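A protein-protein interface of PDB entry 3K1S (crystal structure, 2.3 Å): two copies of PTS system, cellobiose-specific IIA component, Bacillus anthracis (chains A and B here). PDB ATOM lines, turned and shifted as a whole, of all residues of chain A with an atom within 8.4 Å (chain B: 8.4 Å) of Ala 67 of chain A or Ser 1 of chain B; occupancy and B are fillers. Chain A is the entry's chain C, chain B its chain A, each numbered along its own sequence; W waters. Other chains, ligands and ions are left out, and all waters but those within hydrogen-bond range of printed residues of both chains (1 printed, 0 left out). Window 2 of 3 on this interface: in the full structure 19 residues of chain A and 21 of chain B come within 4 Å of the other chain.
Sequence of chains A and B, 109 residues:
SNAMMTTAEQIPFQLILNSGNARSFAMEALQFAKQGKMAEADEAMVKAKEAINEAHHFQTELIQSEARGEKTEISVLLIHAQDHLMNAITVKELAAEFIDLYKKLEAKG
O of Ala 67 of chain A sits at hydrogen-bond distance from N of Asn 2 of chain B (2.8 Å). N of Val 76 of chain B lies within hydrogen-bond range of OE2 of Glu 66 of chain A, at 2.8 Å. The backbone NH (N) of Leu 77 of chain B is in hydrogen-bond range of the side-chain carboxylate (OE1) of Glu 66 of chain A (3.0 Å).
OG of Ser 1 of chain B lies within hydrogen-bond range of O of Met 4 of chain B, 3.1 Å away. The backbone NH of Ser 1 of chain B sits at hydrogen-bond distance from the side-chain carboxylate of Glu 9 of chain B, 3.4 Å away. The side-chain amino group of Lys 71 of chain A lies within salt-bridge range of the side-chain carboxylate of Glu 66 of chain A (3.97 Å).
Val 76 of chain B touches Ile 63 of chain A. Ser 75 of chain B touches Glu 66 of chain A (CB to OE2, 3.1 Å). O of Ala 67 of chain A touches CB of Ser 1 of chain B, 3.7 Å away.
Of the printed residues of chain B, Ile 63 of chain A touches Val 76. Of chain B, only Ser 1 and Asn 2 come within 4 Å of Ala 67 of chain A. Of chain A, only Ala 67 (3.7 Å) comes within 4 Å of Ser 1 of chain B. Of the printed residues of chain A, Ser 75 of chain B touches Glu 66. The nearest printed residue of chain A that does not touch Ser 1 of chain B is Glu 66 of chain A (4.2 Å).
Of the 11 printed residues of chain B, 5 touch a printed residue of chain A. Among the printed residues, no Asp or Glu carboxylate lies within 4 Å of a Lys or Arg side-chain nitrogen of the other chain.
No position is printed for both chains. Of the 6 pairs that touch across the chains among the printed residues, none has its exchanged pair printed and touching as well.
Water W1 lies within hydrogen-bond range of N of Ala 3 of chain B (3.0 Å), O of Ala 67 of chain A (3.2 Å) and O of Arg 68 of chain A (3.3 Å).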
ATOM      1  N   THR A  60      -9.741 -15.377   2.786  1.00  0.00           N
ATOM      2  CA  THR A  60     -10.935 -16.175   3.040  1.00  0.00           C
ATOM      3  C   THR A  60     -11.162 -17.139   1.870  1.00  0.00           C
ATOM      4  O   THR A  60     -11.443 -18.322   2.086  1.00  0.00           O
ATOM      5  CB  THR A  60     -12.181 -15.285   3.283  1.00  0.00           C
ATOM      6  OG1 THR A  60     -11.848 -14.238   4.204  1.00  0.00           O
ATOM      7  CG2 THR A  60     -13.338 -16.097   3.865  1.00  0.00           C
ATOM      8  N   GLU A  61     -11.005 -16.635   0.641  1.00  0.00           N
ATOM      9  CA  GLU A  61     -11.145 -17.455  -0.566  1.00  0.00           C
ATOM     10  C   GLU A  61     -10.065 -18.531  -0.702  1.00  0.00           C
ATOM     11  O   GLU A  61     -10.334 -19.614  -1.226  1.00  0.00           O
ATOM     12  CB  GLU A  61     -11.170 -16.586  -1.826  1.00  0.00           C
ATOM     13  CG  GLU A  61     -11.254 -17.395  -3.128  1.00  0.00           C
ATOM     14  CD  GLU A  61     -12.524 -18.236  -3.236  1.00  0.00           C
ATOM     15  OE1 GLU A  61     -13.506 -17.929  -2.530  1.00  0.00           O
ATOM     16  OE2 GLU A  61     -12.544 -19.207  -4.028  1.00  0.00           O
ATOM     17  N   LEU A  62      -8.847 -18.222  -0.261  1.00  0.00           N
ATOM     18  CA  LEU A  62      -7.758 -19.204  -0.233  1.00  0.00           C
ATOM     19  C   LEU A  62      -8.087 -20.369   0.688  1.00  0.00           C
ATOM     20  O   LEU A  62      -7.976 -21.528   0.287  1.00  0.00           O
ATOM     21  CB  LEU A  62      -6.440 -18.560   0.205  1.00  0.00           C
ATOM     22  CG  LEU A  62      -5.601 -17.886  -0.883  1.00  0.00           C
ATOM     23  CD1 LEU A  62      -4.650 -16.893  -0.260  1.00  0.00           C
ATOM     24  CD2 LEU A  62      -4.837 -18.924  -1.687  1.00  0.00           C
ATOM     25  N   ILE A  63      -8.490 -20.047   1.917  1.00  0.00           N
ATOM     26  CA  ILE A  63      -8.873 -21.049   2.913  1.00  0.00           C
ATOM     27  C   ILE A  63     -10.131 -21.824   2.498  1.00  0.00           C
ATOM     28  O   ILE A  63     -10.161 -23.058   2.588  1.00  0.00           O
ATOM     29  CB  ILE A  63      -9.051 -20.419   4.322  1.00  0.00           C
ATOM     30  CG1 ILE A  63      -7.727 -19.793   4.792  1.00  0.00           C
ATOM     31  CG2 ILE A  63      -9.521 -21.466   5.328  1.00  0.00           C
ATOM     32  CD1 ILE A  63      -7.870 -18.821   5.964  1.00  0.00           C
ATOM     33  N   GLN A  64     -11.155 -21.112   2.025  1.00  0.00           N
ATOM     34  CA  GLN A  64     -12.418 -21.759   1.657  1.00  0.00           C
ATOM     35  C   GLN A  64     -12.278 -22.660   0.423  1.00  0.00           C
ATOM     36  O   GLN A  64     -12.771 -23.790   0.418  1.00  0.00           O
ATOM     37  CB  GLN A  64     -13.539 -20.730   1.479  1.00  0.00           C
ATOM     38  CG  GLN A  64     -14.957 -21.319   1.397  1.00  0.00           C
ATOM     39  CD  GLN A  64     -15.350 -22.220   2.579  1.00  0.00           C
ATOM     40  OE1 GLN A  64     -14.818 -22.111   3.694  1.00  0.00           O
ATOM     41  NE2 GLN A  64     -16.306 -23.103   2.335  1.00  0.00           N
ATOM     42  N   SER A  65     -11.594 -22.169  -0.609  1.00  0.00           N
ATOM     43  CA  SER A  65     -11.361 -22.969  -1.811  1.00  0.00           C
ATOM     44  C   SER A  65     -10.686 -24.302  -1.461  1.00  0.00           C
ATOM     45  O   SER A  65     -11.110 -25.361  -1.934  1.00  0.00           O
ATOM     46  CB  SER A  65     -10.558 -22.182  -2.859  1.00  0.00           C
ATOM     47  OG  SER A  65      -9.337 -21.689  -2.329  1.00  0.00           O
ATOM     48  N   GLU A  66      -9.662 -24.247  -0.608  1.00  0.00           N
ATOM     49  CA  GLU A  66      -8.951 -25.445  -0.153  1.00  0.00           C
ATOM     50  C   GLU A  66      -9.866 -26.392   0.625  1.00  0.00           C
ATOM     51  O   GLU A  66      -9.801 -27.616   0.460  1.00  0.00           O
ATOM     52  CB  GLU A  66      -7.725 -25.061   0.691  1.00  0.00           C
ATOM     53  CG  GLU A  66      -7.101 -26.218   1.472  1.00  0.00           C
ATOM     54  CD  GLU A  66      -5.837 -25.815   2.212  1.00  0.00           C
ATOM     55  OE1 GLU A  66      -5.903 -25.613   3.445  1.00  0.00           O
ATOM     56  OE2 GLU A  66      -4.779 -25.697   1.554  1.00  0.00           O
ATOM     57  N   ALA A  67     -10.713 -25.829   1.487  1.00  0.00           N
ATOM     58  CA  ALA A  67     -11.699 -26.641   2.207  1.00  0.00           C
ATOM     59  C   ALA A  67     -12.616 -27.372   1.218  1.00  0.00           C
ATOM     60  O   ALA A  67     -13.076 -28.479   1.499  1.00  0.00           O
ATOM     61  CB  ALA A  67     -12.519 -25.787   3.170  1.00  0.00           C
ATOM     62  N   ARG A  68     -12.873 -26.742   0.069  1.00  0.00           N
ATOM     63  CA  ARG A  68     -13.691 -27.335  -1.002  1.00  0.00           C
ATOM     64  C   ARG A  68     -12.963 -28.439  -1.781  1.00  0.00           C
ATOM     65  O   ARG A  68     -13.578 -29.136  -2.593  1.00  0.00           O
ATOM     66  CB  ARG A  68     -14.142 -26.261  -2.003  1.00  0.00           C
ATOM     67  CG  ARG A  68     -15.397 -25.494  -1.631  1.00  0.00           C
ATOM     68  CD  ARG A  68     -16.003 -24.785  -2.862  1.00  0.00           C
ATOM     69  NE  ARG A  68     -15.042 -23.920  -3.557  1.00  0.00           N
ATOM     70  CZ  ARG A  68     -14.761 -22.666  -3.207  1.00  0.00           C
ATOM     71  NH1 ARG A  68     -15.359 -22.098  -2.161  1.00  0.00           N
ATOM     72  NH2 ARG A  68     -13.869 -21.978  -3.895  1.00  0.00           N
ATOM     73  N   GLY A  69     -11.658 -28.574  -1.553  1.00  0.00           N
ATOM     74  CA  GLY A  69     -10.836 -29.545  -2.276  1.00  0.00           C
ATOM     75  C   GLY A  69     -10.028 -28.937  -3.409  1.00  0.00           C
ATOM     76  O   GLY A  69      -9.276 -29.639  -4.085  1.00  0.00           O
ATOM     77  N   GLU A  70     -10.179 -27.630  -3.616  1.00  0.00           N
ATOM     78  CA  GLU A  70      -9.442 -26.914  -4.658  1.00  0.00           C
ATOM     79  C   GLU A  70      -8.065 -26.497  -4.151  1.00  0.00           C
ATOM     80  O   GLU A  70      -7.925 -25.498  -3.435  1.00  0.00           O
ATOM     81  CB  GLU A  70     -10.234 -25.691  -5.139  1.00  0.00           C
ATOM     82  CG  GLU A  70     -11.601 -26.023  -5.728  1.00  0.00           C
ATOM     83  CD  GLU A  70     -12.546 -24.830  -5.758  1.00  0.00           C
ATOM     84  OE1 GLU A  70     -12.073 -23.679  -5.660  1.00  0.00           O
ATOM     85  OE2 GLU A  70     -13.769 -25.049  -5.893  1.00  0.00           O
ATOM     86  N   LYS A  71      -7.051 -27.268  -4.531  1.00  0.00           N
ATOM     87  CA  LYS A  71      -5.690 -27.071  -4.044  1.00  0.00           C
ATOM     88  C   LYS A  71      -5.040 -25.813  -4.623  1.00  0.00           C
ATOM     89  O   LYS A  71      -5.147 -25.542  -5.816  1.00  0.00           O
ATOM     90  CB  LYS A  71      -4.835 -28.311  -4.354  1.00  0.00           C
ATOM     91  CG  LYS A  71      -3.466 -28.349  -3.663  1.00  0.00           C
ATOM     92  CD  LYS A  71      -3.565 -28.788  -2.198  1.00  0.00           C
ATOM     93  CE  LYS A  71      -2.293 -28.437  -1.419  1.00  0.00           C
ATOM     94  NZ  LYS A  71      -2.173 -26.968  -1.152  1.00  0.00           N
ATOM     95  N   THR A  72      -4.379 -25.047  -3.759  1.00  0.00           N
ATOM     96  CA  THR A  72      -3.569 -23.912  -4.183  1.00  0.00           C
ATOM     97  C   THR A  72      -2.106 -24.329  -4.282  1.00  0.00           C
ATOM     98  O   THR A  72      -1.621 -25.127  -3.478  1.00  0.00           O
ATOM     99  CB  THR A  72      -3.717 -22.721  -3.217  1.00  0.00           C
ATOM    100  OG1 THR A  72      -4.961 -22.058  -3.470  1.00  0.00           O
ATOM    101  CG2 THR A  72      -2.584 -21.716  -3.397  1.00  0.00           C
ATOM    102  N   SER B   1      -9.768 -31.623   3.980  1.00  0.00           N
ATOM    103  CA  SER B   1     -10.870 -30.956   3.230  1.00  0.00           C
ATOM    104  C   SER B   1     -12.229 -31.248   3.865  1.00  0.00           C
ATOM    105  O   SER B   1     -12.335 -32.083   4.770  1.00  0.00           O
ATOM    106  CB  SER B   1     -10.868 -31.426   1.774  1.00  0.00           C
ATOM    107  OG  SER B   1     -11.284 -32.777   1.689  1.00  0.00           O
ATOM    108  N   ASN B   2     -13.266 -30.564   3.383  1.00  0.00           N
ATOM    109  CA  ASN B   2     -14.638 -30.807   3.843  1.00  0.00           C
ATOM    110  C   ASN B   2     -15.146 -32.223   3.552  1.00  0.00           C
ATOM    111  O   ASN B   2     -15.930 -32.776   4.324  1.00  0.00           O
ATOM    112  CB  ASN B   2     -15.601 -29.773   3.251  1.00  0.00           C
ATOM    113  CG  ASN B   2     -15.309 -28.363   3.720  1.00  0.00           C
ATOM    114  OD1 ASN B   2     -14.496 -28.149   4.626  1.00  0.00           O
ATOM    115  ND2 ASN B   2     -15.966 -27.385   3.095  1.00  0.00           N
ATOM    116  N   ALA B   3     -14.708 -32.802   2.437  1.00  0.00           N
ATOM    117  CA  ALA B   3     -15.094 -34.167   2.085  1.00  0.00           C
ATOM    118  C   ALA B   3     -14.419 -35.183   3.006  1.00  0.00           C
ATOM    119  O   ALA B   3     -15.067 -36.115   3.492  1.00  0.00           O
ATOM    120  CB  ALA B   3     -14.766 -34.463   0.630  1.00  0.00           C
ATOM    121  N   MET B   4     -13.122 -34.995   3.243  1.00  0.00           N
ATOM    122  CA  MET B   4     -12.351 -35.902   4.088  1.00  0.00           C
ATOM    123  C   MET B   4     -11.226 -35.175   4.817  1.00  0.00           C
ATOM    124  O   MET B   4     -10.429 -34.465   4.199  1.00  0.00           O
ATOM    125  CB  MET B   4     -11.783 -37.065   3.258  1.00  0.00           C
ATOM    126  CG  MET B   4     -11.161 -38.203   4.083  1.00  0.00           C
ATOM    127  SD  MET B   4     -12.453 -39.151   5.221  1.00  0.00           S
ATOM    128  CE  MET B   4     -11.221 -40.380   6.115  1.00  0.00           C
ATOM    129  N   MET B   5     -11.176 -35.356   6.134  1.00  0.00           N
ATOM    130  CA  MET B   5     -10.054 -34.872   6.933  1.00  0.00           C
ATOM    131  C   MET B   5      -9.179 -36.038   7.390  1.00  0.00           C
ATOM    132  O   MET B   5      -9.654 -36.961   8.060  1.00  0.00           O
ATOM    133  CB  MET B   5     -10.532 -34.057   8.141  1.00  0.00           C
ATOM    134  CG  MET B   5      -9.393 -33.588   9.054  1.00  0.00           C
ATOM    135  SD  MET B   5      -9.974 -32.668  10.679  1.00  0.00           S
ATOM    136  CE  MET B   5      -8.327 -32.861  11.713  1.00  0.00           C
ATOM    137  N   THR B   6      -7.904 -35.986   7.013  1.00  0.00           N
ATOM    138  CA  THR B   6      -6.910 -36.954   7.477  1.00  0.00           C
ATOM    139  C   THR B   6      -6.449 -36.605   8.892  1.00  0.00           C
ATOM    140  O   THR B   6      -6.657 -35.477   9.361  1.00  0.00           O
ATOM    141  CB  THR B   6      -5.676 -36.998   6.545  1.00  0.00           C
ATOM    142  OG1 THR B   6      -4.984 -35.742   6.597  1.00  0.00           O
ATOM    143  CG2 THR B   6      -6.093 -37.301   5.100  1.00  0.00           C
ATOM    144  N   GLU B   9      -4.102 -33.754   9.076  1.00  0.00           N
ATOM    145  CA  GLU B   9      -4.846 -32.513   8.836  1.00  0.00           C
ATOM    146  C   GLU B   9      -5.518 -31.965  10.102  1.00  0.00           C
ATOM    147  O   GLU B   9      -6.079 -30.867  10.089  1.00  0.00           O
ATOM    148  CB  GLU B   9      -5.863 -32.694   7.699  1.00  0.00           C
ATOM    149  CG  GLU B   9      -5.214 -32.951   6.337  1.00  0.00           C
ATOM    150  CD  GLU B   9      -6.207 -33.026   5.180  1.00  0.00           C
ATOM    151  OE1 GLU B   9      -7.344 -33.515   5.370  1.00  0.00           O
ATOM    152  OE2 GLU B   9      -5.836 -32.603   4.065  1.00  0.00           O
ATOM    153  N   PHE B  13      -5.978 -27.386  12.813  1.00  0.00           N
ATOM    154  CA  PHE B  13      -7.155 -27.046  13.634  1.00  0.00           C
ATOM    155  C   PHE B  13      -6.833 -26.900  15.127  1.00  0.00           C
ATOM    156  O   PHE B  13      -7.348 -25.996  15.794  1.00  0.00           O
ATOM    157  CB  PHE B  13      -8.278 -28.071  13.448  1.00  0.00           C
ATOM    158  CG  PHE B  13      -8.905 -28.055  12.078  1.00  0.00           C
ATOM    159  CD1 PHE B  13      -9.831 -27.073  11.729  1.00  0.00           C
ATOM    160  CD2 PHE B  13      -8.581 -29.034  11.138  1.00  0.00           C
ATOM    161  CE1 PHE B  13     -10.420 -27.060  10.471  1.00  0.00           C
ATOM    162  CE2 PHE B  13      -9.162 -29.028   9.866  1.00  0.00           C
ATOM    163  CZ  PHE B  13     -10.089 -28.044   9.538  1.00  0.00           C
ATOM    164  N   SER B  75      -0.347 -26.903   3.301  1.00  0.00           N
ATOM    165  CA  SER B  75      -1.638 -26.386   2.863  1.00  0.00           C
ATOM    166  C   SER B  75      -1.801 -24.952   3.353  1.00  0.00           C
ATOM    167  O   SER B  75      -1.066 -24.509   4.238  1.00  0.00           O
ATOM    168  CB  SER B  75      -2.778 -27.259   3.401  1.00  0.00           C
ATOM    169  OG  SER B  75      -2.856 -27.185   4.824  1.00  0.00           O
ATOM    170  N   VAL B  76      -2.753 -24.227   2.770  1.00  0.00           N
ATOM    171  CA  VAL B  76      -3.094 -22.895   3.262  1.00  0.00           C
ATOM    172  C   VAL B  76      -3.406 -22.937   4.766  1.00  0.00           C
ATOM    173  O   VAL B  76      -2.908 -22.098   5.523  1.00  0.00           O
ATOM    174  CB  VAL B  76      -4.265 -22.268   2.473  1.00  0.00           C
ATOM    175  CG1 VAL B  76      -4.731 -20.992   3.137  1.00  0.00           C
ATOM    176  CG2 VAL B  76      -3.853 -21.992   1.009  1.00  0.00           C
ATOM    177  N   LEU B  77      -4.201 -23.916   5.198  1.00  0.00           N
ATOM    178  CA  LEU B  77      -4.612 -23.991   6.606  1.00  0.00           C
ATOM    179  C   LEU B  77      -3.419 -24.181   7.548  1.00  0.00           C
ATOM    180  O   LEU B  77      -3.340 -23.523   8.576  1.00  0.00           O
ATOM    181  CB  LEU B  77      -5.698 -25.061   6.854  1.00  0.00           C
ATOM    182  CG  LEU B  77      -6.465 -24.910   8.186  1.00  0.00           C
ATOM    183  CD1 LEU B  77      -7.271 -23.613   8.227  1.00  0.00           C
ATOM    184  CD2 LEU B  77      -7.368 -26.107   8.490  1.00  0.00           C
HETATM  185  O   HOH W   1     -14.119 -31.108  -0.018  1.00  0.00           O
